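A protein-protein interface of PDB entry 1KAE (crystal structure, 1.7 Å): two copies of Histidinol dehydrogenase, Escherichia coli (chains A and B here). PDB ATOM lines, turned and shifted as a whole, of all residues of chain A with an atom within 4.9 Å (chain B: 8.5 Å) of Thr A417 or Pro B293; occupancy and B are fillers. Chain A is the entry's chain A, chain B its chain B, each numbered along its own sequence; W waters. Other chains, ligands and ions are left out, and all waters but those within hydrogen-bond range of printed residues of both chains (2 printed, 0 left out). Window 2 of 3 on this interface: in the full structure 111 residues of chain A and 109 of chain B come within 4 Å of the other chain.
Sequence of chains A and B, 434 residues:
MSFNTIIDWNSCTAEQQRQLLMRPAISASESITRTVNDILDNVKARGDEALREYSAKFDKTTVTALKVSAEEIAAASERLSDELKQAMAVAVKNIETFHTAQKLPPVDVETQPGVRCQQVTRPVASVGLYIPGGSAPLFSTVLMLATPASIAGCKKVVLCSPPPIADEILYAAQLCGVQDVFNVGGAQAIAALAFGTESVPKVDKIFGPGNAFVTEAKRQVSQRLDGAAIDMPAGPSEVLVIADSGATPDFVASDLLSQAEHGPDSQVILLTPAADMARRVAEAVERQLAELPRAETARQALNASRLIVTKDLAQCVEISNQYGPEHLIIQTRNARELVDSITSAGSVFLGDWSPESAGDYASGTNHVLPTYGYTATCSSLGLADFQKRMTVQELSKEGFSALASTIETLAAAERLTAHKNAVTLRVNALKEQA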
ATOM      1  N   ARG A 415      19.477  17.986   4.253  1.00  0.00           N
ATOM      2  CA  ARG A 415      18.291  18.842   4.191  1.00  0.00           C
ATOM      3  C   ARG A 415      18.596  20.297   3.834  1.00  0.00           C
ATOM      4  O   ARG A 415      17.998  21.227   4.406  1.00  0.00           O
ATOM      5  CB  ARG A 415      17.490  18.770   5.501  1.00  0.00           C
ATOM      6  CG  ARG A 415      17.153  17.340   5.879  1.00  0.00           C
ATOM      7  CD  ARG A 415      16.165  17.251   7.056  1.00  0.00           C
ATOM      8  NE  ARG A 415      16.103  15.869   7.563  1.00  0.00           N
ATOM      9  CZ  ARG A 415      15.630  15.515   8.760  1.00  0.00           C
ATOM     10  NH1 ARG A 415      15.160  16.436   9.596  1.00  0.00           N
ATOM     11  NH2 ARG A 415      15.654  14.241   9.131  1.00  0.00           N
ATOM     12  N   LEU A 416      19.528  20.498   2.898  1.00  0.00           N
ATOM     13  CA  LEU A 416      19.896  21.843   2.466  1.00  0.00           C
ATOM     14  C   LEU A 416      19.363  21.992   1.045  1.00  0.00           C
ATOM     15  O   LEU A 416      20.069  21.772   0.047  1.00  0.00           O
ATOM     16  CB  LEU A 416      21.408  22.020   2.546  1.00  0.00           C
ATOM     17  CG  LEU A 416      21.922  22.130   4.017  1.00  0.00           C
ATOM     18  CD1 LEU A 416      23.410  22.272   4.096  1.00  0.00           C
ATOM     19  CD2 LEU A 416      21.301  23.391   4.675  1.00  0.00           C
ATOM     20  N   THR A 417      18.105  22.367   0.955  1.00  0.00           N
ATOM     21  CA  THR A 417      17.423  22.470  -0.323  1.00  0.00           C
ATOM     22  C   THR A 417      18.016  23.482  -1.266  1.00  0.00           C
ATOM     23  O   THR A 417      18.106  23.232  -2.477  1.00  0.00           O
ATOM     24  CB  THR A 417      15.937  22.773  -0.108  1.00  0.00           C
ATOM     25  OG1 THR A 417      15.391  21.758   0.742  1.00  0.00           O
ATOM     26  CG2 THR A 417      15.177  22.756  -1.433  1.00  0.00           C
ATOM     27  N   ALA A 418      18.391  24.644  -0.750  1.00  0.00           N
ATOM     28  CA  ALA A 418      18.978  25.634  -1.644  1.00  0.00           C
ATOM     29  C   ALA A 418      20.274  25.114  -2.284  1.00  0.00           C
ATOM     30  O   ALA A 418      20.542  25.416  -3.469  1.00  0.00           O
ATOM     31  CB  ALA A 418      19.223  26.958  -0.892  1.00  0.00           C
ATOM     32  N   HIS A 419      21.089  24.389  -1.516  1.00  0.00           N
ATOM     33  CA  HIS A 419      22.339  23.809  -2.032  1.00  0.00           C
ATOM     34  C   HIS A 419      21.994  22.835  -3.150  1.00  0.00           C
ATOM     35  O   HIS A 419      22.687  22.801  -4.180  1.00  0.00           O
ATOM     36  CB  HIS A 419      23.122  23.035  -0.936  1.00  0.00           C
ATOM     37  CG  HIS A 419      23.922  23.901  -0.003  1.00  0.00           C
ATOM     38  ND1 HIS A 419      23.338  24.741   0.930  1.00  0.00           N
ATOM     39  CD2 HIS A 419      25.260  23.993   0.200  1.00  0.00           C
ATOM     40  CE1 HIS A 419      24.280  25.312   1.662  1.00  0.00           C
ATOM     41  NE2 HIS A 419      25.456  24.880   1.240  1.00  0.00           N
ATOM     42  N   LYS A 420      20.939  22.033  -2.943  1.00  0.00           N
ATOM     43  CA  LYS A 420      20.494  21.049  -3.930  1.00  0.00           C
ATOM     44  C   LYS A 420      19.940  21.792  -5.141  1.00  0.00           C
ATOM     45  O   LYS A 420      20.302  21.474  -6.293  1.00  0.00           O
ATOM     46  CB  LYS A 420      19.414  20.145  -3.313  1.00  0.00           C
ATOM     47  CG  LYS A 420      18.890  19.038  -4.240  1.00  0.00           C
ATOM     48  CD  LYS A 420      17.798  18.234  -3.486  1.00  0.00           C
ATOM     49  CE  LYS A 420      17.257  17.134  -4.355  1.00  0.00           C
ATOM     50  NZ  LYS A 420      16.622  17.685  -5.576  1.00  0.00           N
ATOM     51  N   ASN A 421      19.080  22.797  -4.912  1.00  0.00           N
ATOM     52  CA  ASN A 421      18.527  23.557  -6.043  1.00  0.00           C
ATOM     53  C   ASN A 421      19.564  24.236  -6.955  1.00  0.00           C
ATOM     54  O   ASN A 421      19.299  24.382  -8.151  1.00  0.00           O
ATOM     55  CB  ASN A 421      17.562  24.646  -5.579  1.00  0.00           C
ATOM     56  CG  ASN A 421      16.274  24.099  -4.995  1.00  0.00           C
ATOM     57  OD1 ASN A 421      15.927  22.887  -5.072  1.00  0.00           O
ATOM     58  ND2 ASN A 421      15.523  25.013  -4.403  1.00  0.00           N
ATOM     59  N   SER B 254      20.932  31.336  -6.893  1.00  0.00           N
ATOM     60  CA  SER B 254      20.975  30.044  -6.211  1.00  0.00           C
ATOM     61  C   SER B 254      22.221  29.867  -5.314  1.00  0.00           C
ATOM     62  O   SER B 254      22.167  29.178  -4.280  1.00  0.00           O
ATOM     63  CB  SER B 254      20.885  28.908  -7.236  1.00  0.00           C
ATOM     64  OG  SER B 254      22.123  28.733  -7.899  1.00  0.00           O
ATOM     65  N   LEU B 257      21.548  32.108  -2.219  1.00  0.00           N
ATOM     66  CA  LEU B 257      20.654  31.366  -1.330  1.00  0.00           C
ATOM     67  C   LEU B 257      21.282  30.120  -0.732  1.00  0.00           C
ATOM     68  O   LEU B 257      20.914  29.762   0.381  1.00  0.00           O
ATOM     69  CB  LEU B 257      19.361  30.968  -2.038  1.00  0.00           C
ATOM     70  CG  LEU B 257      18.424  32.170  -2.088  1.00  0.00           C
ATOM     71  CD1 LEU B 257      17.326  32.026  -3.172  1.00  0.00           C
ATOM     72  CD2 LEU B 257      17.825  32.238  -0.658  1.00  0.00           C
ATOM     73  N   SER B 258      22.196  29.425  -1.434  1.00  0.00           N
ATOM     74  CA  SER B 258      22.801  28.240  -0.765  1.00  0.00           C
ATOM     75  C   SER B 258      23.499  28.685   0.489  1.00  0.00           C
ATOM     76  O   SER B 258      23.421  28.059   1.537  1.00  0.00           O
ATOM     77  CB  SER B 258      23.820  27.475  -1.663  1.00  0.00           C
ATOM     78  OG  SER B 258      24.679  28.320  -2.416  1.00  0.00           O
ATOM     79  N   GLU B 261      20.907  30.036   3.425  1.00  0.00           N
ATOM     80  CA  GLU B 261      20.186  28.998   4.185  1.00  0.00           C
ATOM     81  C   GLU B 261      20.974  28.334   5.298  1.00  0.00           C
ATOM     82  O   GLU B 261      20.393  27.615   6.122  1.00  0.00           O
ATOM     83  CB  GLU B 261      19.626  27.904   3.239  1.00  0.00           C
ATOM     84  CG  GLU B 261      20.635  26.848   2.809  1.00  0.00           C
ATOM     85  CD  GLU B 261      19.958  25.732   2.021  1.00  0.00           C
ATOM     86  OE1 GLU B 261      18.701  25.710   1.926  1.00  0.00           O
ATOM     87  OE2 GLU B 261      20.674  24.869   1.483  1.00  0.00           O
ATOM     88  N   GLN B 288      13.162  32.458  -5.868  1.00  0.00           N
ATOM     89  CA  GLN B 288      13.690  31.198  -5.370  1.00  0.00           C
ATOM     90  C   GLN B 288      13.464  31.036  -3.889  1.00  0.00           C
ATOM     91  O   GLN B 288      13.151  29.946  -3.403  1.00  0.00           O
ATOM     92  CB  GLN B 288      15.200  31.063  -5.689  1.00  0.00           C
ATOM     93  CG  GLN B 288      15.459  30.817  -7.185  1.00  0.00           C
ATOM     94  CD  GLN B 288      16.933  30.615  -7.492  1.00  0.00           C
ATOM     95  OE1 GLN B 288      17.642  30.088  -6.669  1.00  0.00           O
ATOM     96  NE2 GLN B 288      17.380  31.017  -8.692  1.00  0.00           N
ATOM     97  N   LEU B 289      13.588  32.136  -3.153  1.00  0.00           N
ATOM     98  CA  LEU B 289      13.386  32.078  -1.700  1.00  0.00           C
ATOM     99  C   LEU B 289      11.973  31.569  -1.387  1.00  0.00           C
ATOM    100  O   LEU B 289      11.788  30.758  -0.471  1.00  0.00           O
ATOM    101  CB  LEU B 289      13.569  33.493  -1.112  1.00  0.00           C
ATOM    102  CG  LEU B 289      13.314  33.639   0.379  1.00  0.00           C
ATOM    103  CD1 LEU B 289      14.249  32.809   1.173  1.00  0.00           C
ATOM    104  CD2 LEU B 289      13.382  35.112   0.739  1.00  0.00           C
ATOM    105  N   ALA B 290      10.996  32.052  -2.155  1.00  0.00           N
ATOM    106  CA  ALA B 290       9.573  31.710  -1.958  1.00  0.00           C
ATOM    107  C   ALA B 290       9.338  30.221  -2.010  1.00  0.00           C
ATOM    108  O   ALA B 290       8.405  29.715  -1.377  1.00  0.00           O
ATOM    109  CB  ALA B 290       8.681  32.461  -3.013  1.00  0.00           C
ATOM    110  N   GLU B 291      10.196  29.500  -2.737  1.00  0.00           N
ATOM    111  CA  GLU B 291      10.085  28.039  -2.854  1.00  0.00           C
ATOM    112  C   GLU B 291      10.878  27.207  -1.847  1.00  0.00           C
ATOM    113  O   GLU B 291      10.791  25.972  -1.884  1.00  0.00           O
ATOM    114  CB  GLU B 291      10.555  27.566  -4.248  1.00  0.00           C
ATOM    115  CG  GLU B 291       9.725  28.033  -5.361  1.00  0.00           C
ATOM    116  CD  GLU B 291       9.997  27.272  -6.621  1.00  0.00           C
ATOM    117  OE1 GLU B 291       9.709  26.080  -6.643  1.00  0.00           O
ATOM    118  OE2 GLU B 291      10.480  27.848  -7.596  1.00  0.00           O
ATOM    119  N   LEU B 292      11.659  27.828  -0.966  1.00  0.00           N
ATOM    120  CA  LEU B 292      12.461  27.049  -0.029  1.00  0.00           C
ATOM    121  C   LEU B 292      11.644  26.547   1.134  1.00  0.00           C
ATOM    122  O   LEU B 292      11.061  27.359   1.876  1.00  0.00           O
ATOM    123  CB  LEU B 292      13.655  27.860   0.490  1.00  0.00           C
ATOM    124  CG  LEU B 292      14.720  28.256  -0.515  1.00  0.00           C
ATOM    125  CD1 LEU B 292      15.793  29.137   0.196  1.00  0.00           C
ATOM    126  CD2 LEU B 292      15.376  26.997  -1.092  1.00  0.00           C
ATOM    127  N   PRO B 293      11.617  25.204   1.331  1.00  0.00           N
ATOM    128  CA  PRO B 293      10.909  24.416   2.355  1.00  0.00           C
ATOM    129  C   PRO B 293      10.883  25.044   3.727  1.00  0.00           C
ATOM    130  O   PRO B 293       9.903  24.879   4.493  1.00  0.00           O
ATOM    131  CB  PRO B 293      11.676  23.092   2.363  1.00  0.00           C
ATOM    132  CG  PRO B 293      11.993  22.924   0.976  1.00  0.00           C
ATOM    133  CD  PRO B 293      12.486  24.305   0.547  1.00  0.00           C
ATOM    134  N   ARG B 294      11.961  25.763   4.024  1.00  0.00           N
ATOM    135  CA  ARG B 294      12.128  26.404   5.305  1.00  0.00           C
ATOM    136  C   ARG B 294      13.094  27.538   5.037  1.00  0.00           C
ATOM    137  O   ARG B 294      14.304  27.418   5.269  1.00  0.00           O
ATOM    138  CB  ARG B 294      12.723  25.401   6.300  1.00  0.00           C
ATOM    139  N   ALA B 295      12.515  28.615   4.504  1.00  0.00           N
ATOM    140  CA  ALA B 295      13.149  29.860   4.093  1.00  0.00           C
ATOM    141  C   ALA B 295      13.181  30.929   5.197  1.00  0.00           C
ATOM    142  O   ALA B 295      13.479  32.088   4.903  1.00  0.00           O
ATOM    143  CB  ALA B 295      12.376  30.442   2.904  1.00  0.00           C
ATOM    144  N   GLU B 296      12.838  30.568   6.432  1.00  0.00           N
ATOM    145  CA  GLU B 296      12.825  31.574   7.504  1.00  0.00           C
ATOM    146  C   GLU B 296      14.245  32.027   7.781  1.00  0.00           C
ATOM    147  O   GLU B 296      14.523  33.236   7.920  1.00  0.00           O
ATOM    148  CB  GLU B 296      12.199  31.021   8.779  1.00  0.00           C
ATOM    149  CG  GLU B 296      10.708  30.725   8.670  1.00  0.00           C
ATOM    150  CD  GLU B 296      10.164  30.099   9.943  1.00  0.00           C
ATOM    151  OE1 GLU B 296      10.920  29.344  10.595  1.00  0.00           O
ATOM    152  OE2 GLU B 296       8.989  30.344  10.289  1.00  0.00           O
ATOM    153  N   THR B 297      15.136  31.051   7.860  1.00  0.00           N
ATOM    154  CA  THR B 297      16.542  31.317   8.086  1.00  0.00           C
ATOM    155  C   THR B 297      17.173  32.104   6.929  1.00  0.00           C
ATOM    156  O   THR B 297      17.931  33.035   7.156  1.00  0.00           O
ATOM    157  CB  THR B 297      17.341  30.030   8.221  1.00  0.00           C
ATOM    158  OG1 THR B 297      16.915  29.323   9.379  1.00  0.00           O
ATOM    159  CG2 THR B 297      18.792  30.342   8.379  1.00  0.00           C
ATOM    160  N   SER B 357      27.828  24.615  -3.851  1.00  0.00           N
ATOM    161  CA  SER B 357      27.441  23.234  -3.488  1.00  0.00           C
ATOM    162  C   SER B 357      28.469  22.222  -3.967  1.00  0.00           C
ATOM    163  O   SER B 357      28.758  21.241  -3.256  1.00  0.00           O
ATOM    164  CB  SER B 357      26.072  22.843  -4.123  1.00  0.00           C
ATOM    165  OG  SER B 357      25.157  23.877  -3.930  1.00  0.00           O
ATOM    166  N   TYR B 361      30.445  19.848  -1.053  1.00  0.00           N
ATOM    167  CA  TYR B 361      30.291  18.394  -1.036  1.00  0.00           C
ATOM    168  C   TYR B 361      31.229  17.456  -1.764  1.00  0.00           C
ATOM    169  O   TYR B 361      31.592  16.426  -1.197  1.00  0.00           O
ATOM    170  CB  TYR B 361      28.894  18.038  -1.540  1.00  0.00           C
ATOM    171  CG  TYR B 361      27.802  18.533  -0.647  1.00  0.00           C
ATOM    172  CD1 TYR B 361      26.957  19.567  -1.043  1.00  0.00           C
ATOM    173  CD2 TYR B 361      27.628  17.963   0.623  1.00  0.00           C
ATOM    174  CE1 TYR B 361      25.949  20.034  -0.179  1.00  0.00           C
ATOM    175  CE2 TYR B 361      26.627  18.409   1.474  1.00  0.00           C
ATOM    176  CZ  TYR B 361      25.795  19.442   1.079  1.00  0.00           C
ATOM    177  OH  TYR B 361      24.820  19.883   1.953  1.00  0.00           O
HETATM  178  O   HOH W   1      19.872  27.721  -4.236  1.00  0.00           O
HETATM  179  O   HOH W   2      12.752  24.595  -3.500  1.00  0.00           O
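Hydrophobic or aromatic side chains of chain A within 4 Å of the printed part of chain B: Leu A416, Ala A418 and His A419.
Of the 16 printed residues of chain B, 7 touch a printed residue of chain A.
Printed residues of chain B that touch a printed residue of chain A: Leu B257, Ser B258, Glu B261, Leu B292, Pro B293, Ser B357 and Tyr B361.
Hydrophobic or aromatic side chains of chain B within 4 Å of the printed part of chain A: Leu B292, Pro B293 and Tyr B361.
Among the printed residues, 12 pairs touch across the chains.
Of the printed residues of chain B, Leu A416 touches Glu B261 and Tyr B361.
Of chain B, only Glu B261 and Pro B293 come within 4 Å of Thr A417.
Printed residues of chain B within 4 Å of His A419: Ser B258, Glu B261 and Ser B357.
Ala B290 touches none of the printed residues of chain A.
Of the printed residues of chain A, Leu B292 touches Ala A418 (3.8 Å) and Asn A421 (3.9 Å).
Of chain A, only Thr A417 comes within 4 Å of Pro B293.
Thr B297 touches none of the printed residues of chain A.
The nearest printed residue of chain A that does not touch Pro B293 is Asn A421 (5.9 Å).
ND1 of His A419 lies close to O of Ser B258, at 3.4 Å.
The backbone NH of Ala A418 is in hydrogen-bond range of the side-chain carboxylate of Glu B261 (2.9 Å).
O of Leu A416 lies close to OE2 of Glu B261, 3.5 Å away.
ND1 of His A419 lies within hydrogen-bond range of OE2 of Glu B261 (2.7 Å).
The backbone carbonyl oxygen of His A419 is in hydrogen-bond range of the side-chain hydroxyl of Ser B357, at 2.7 Å.
Among the printed residues, pairs that only touch across the chains: Leu A416 with Tyr B361 (3.5 Å), Ala A418 with Leu B257 (3.5 Å), Thr A417 with Glu B261 (3.5 Å), Thr A417 with Pro B293 (3.6 Å), Ala A418 with Ser B258 (3.8 Å), Ala A418 with Leu B292 (3.8 Å) and Asn A421 with Leu B292 (3.9 Å).
No position is printed for both chains.
Of the 12 pairs that touch across the chains among the printed residues, none has its exchanged pair printed and touching as well.
Water W1 bridges O of Ala A418 (2.5 Å) and O of Ser B254 (2.7 Å).
Water W2 bridges the backbone carbonyl oxygen of Glu B291 (2.9 Å) and the side-chain amide nitrogen of Asn A421 (2.9 Å).
O of Ser B254 lies within hydrogen-bond range of OG of Ser B258, 3.2 Å away.
The backbone carbonyl oxygen (O) of Thr A417 lies close to the side-chain amide oxygen (OD1) of Asn A421, 3.4 Å away.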
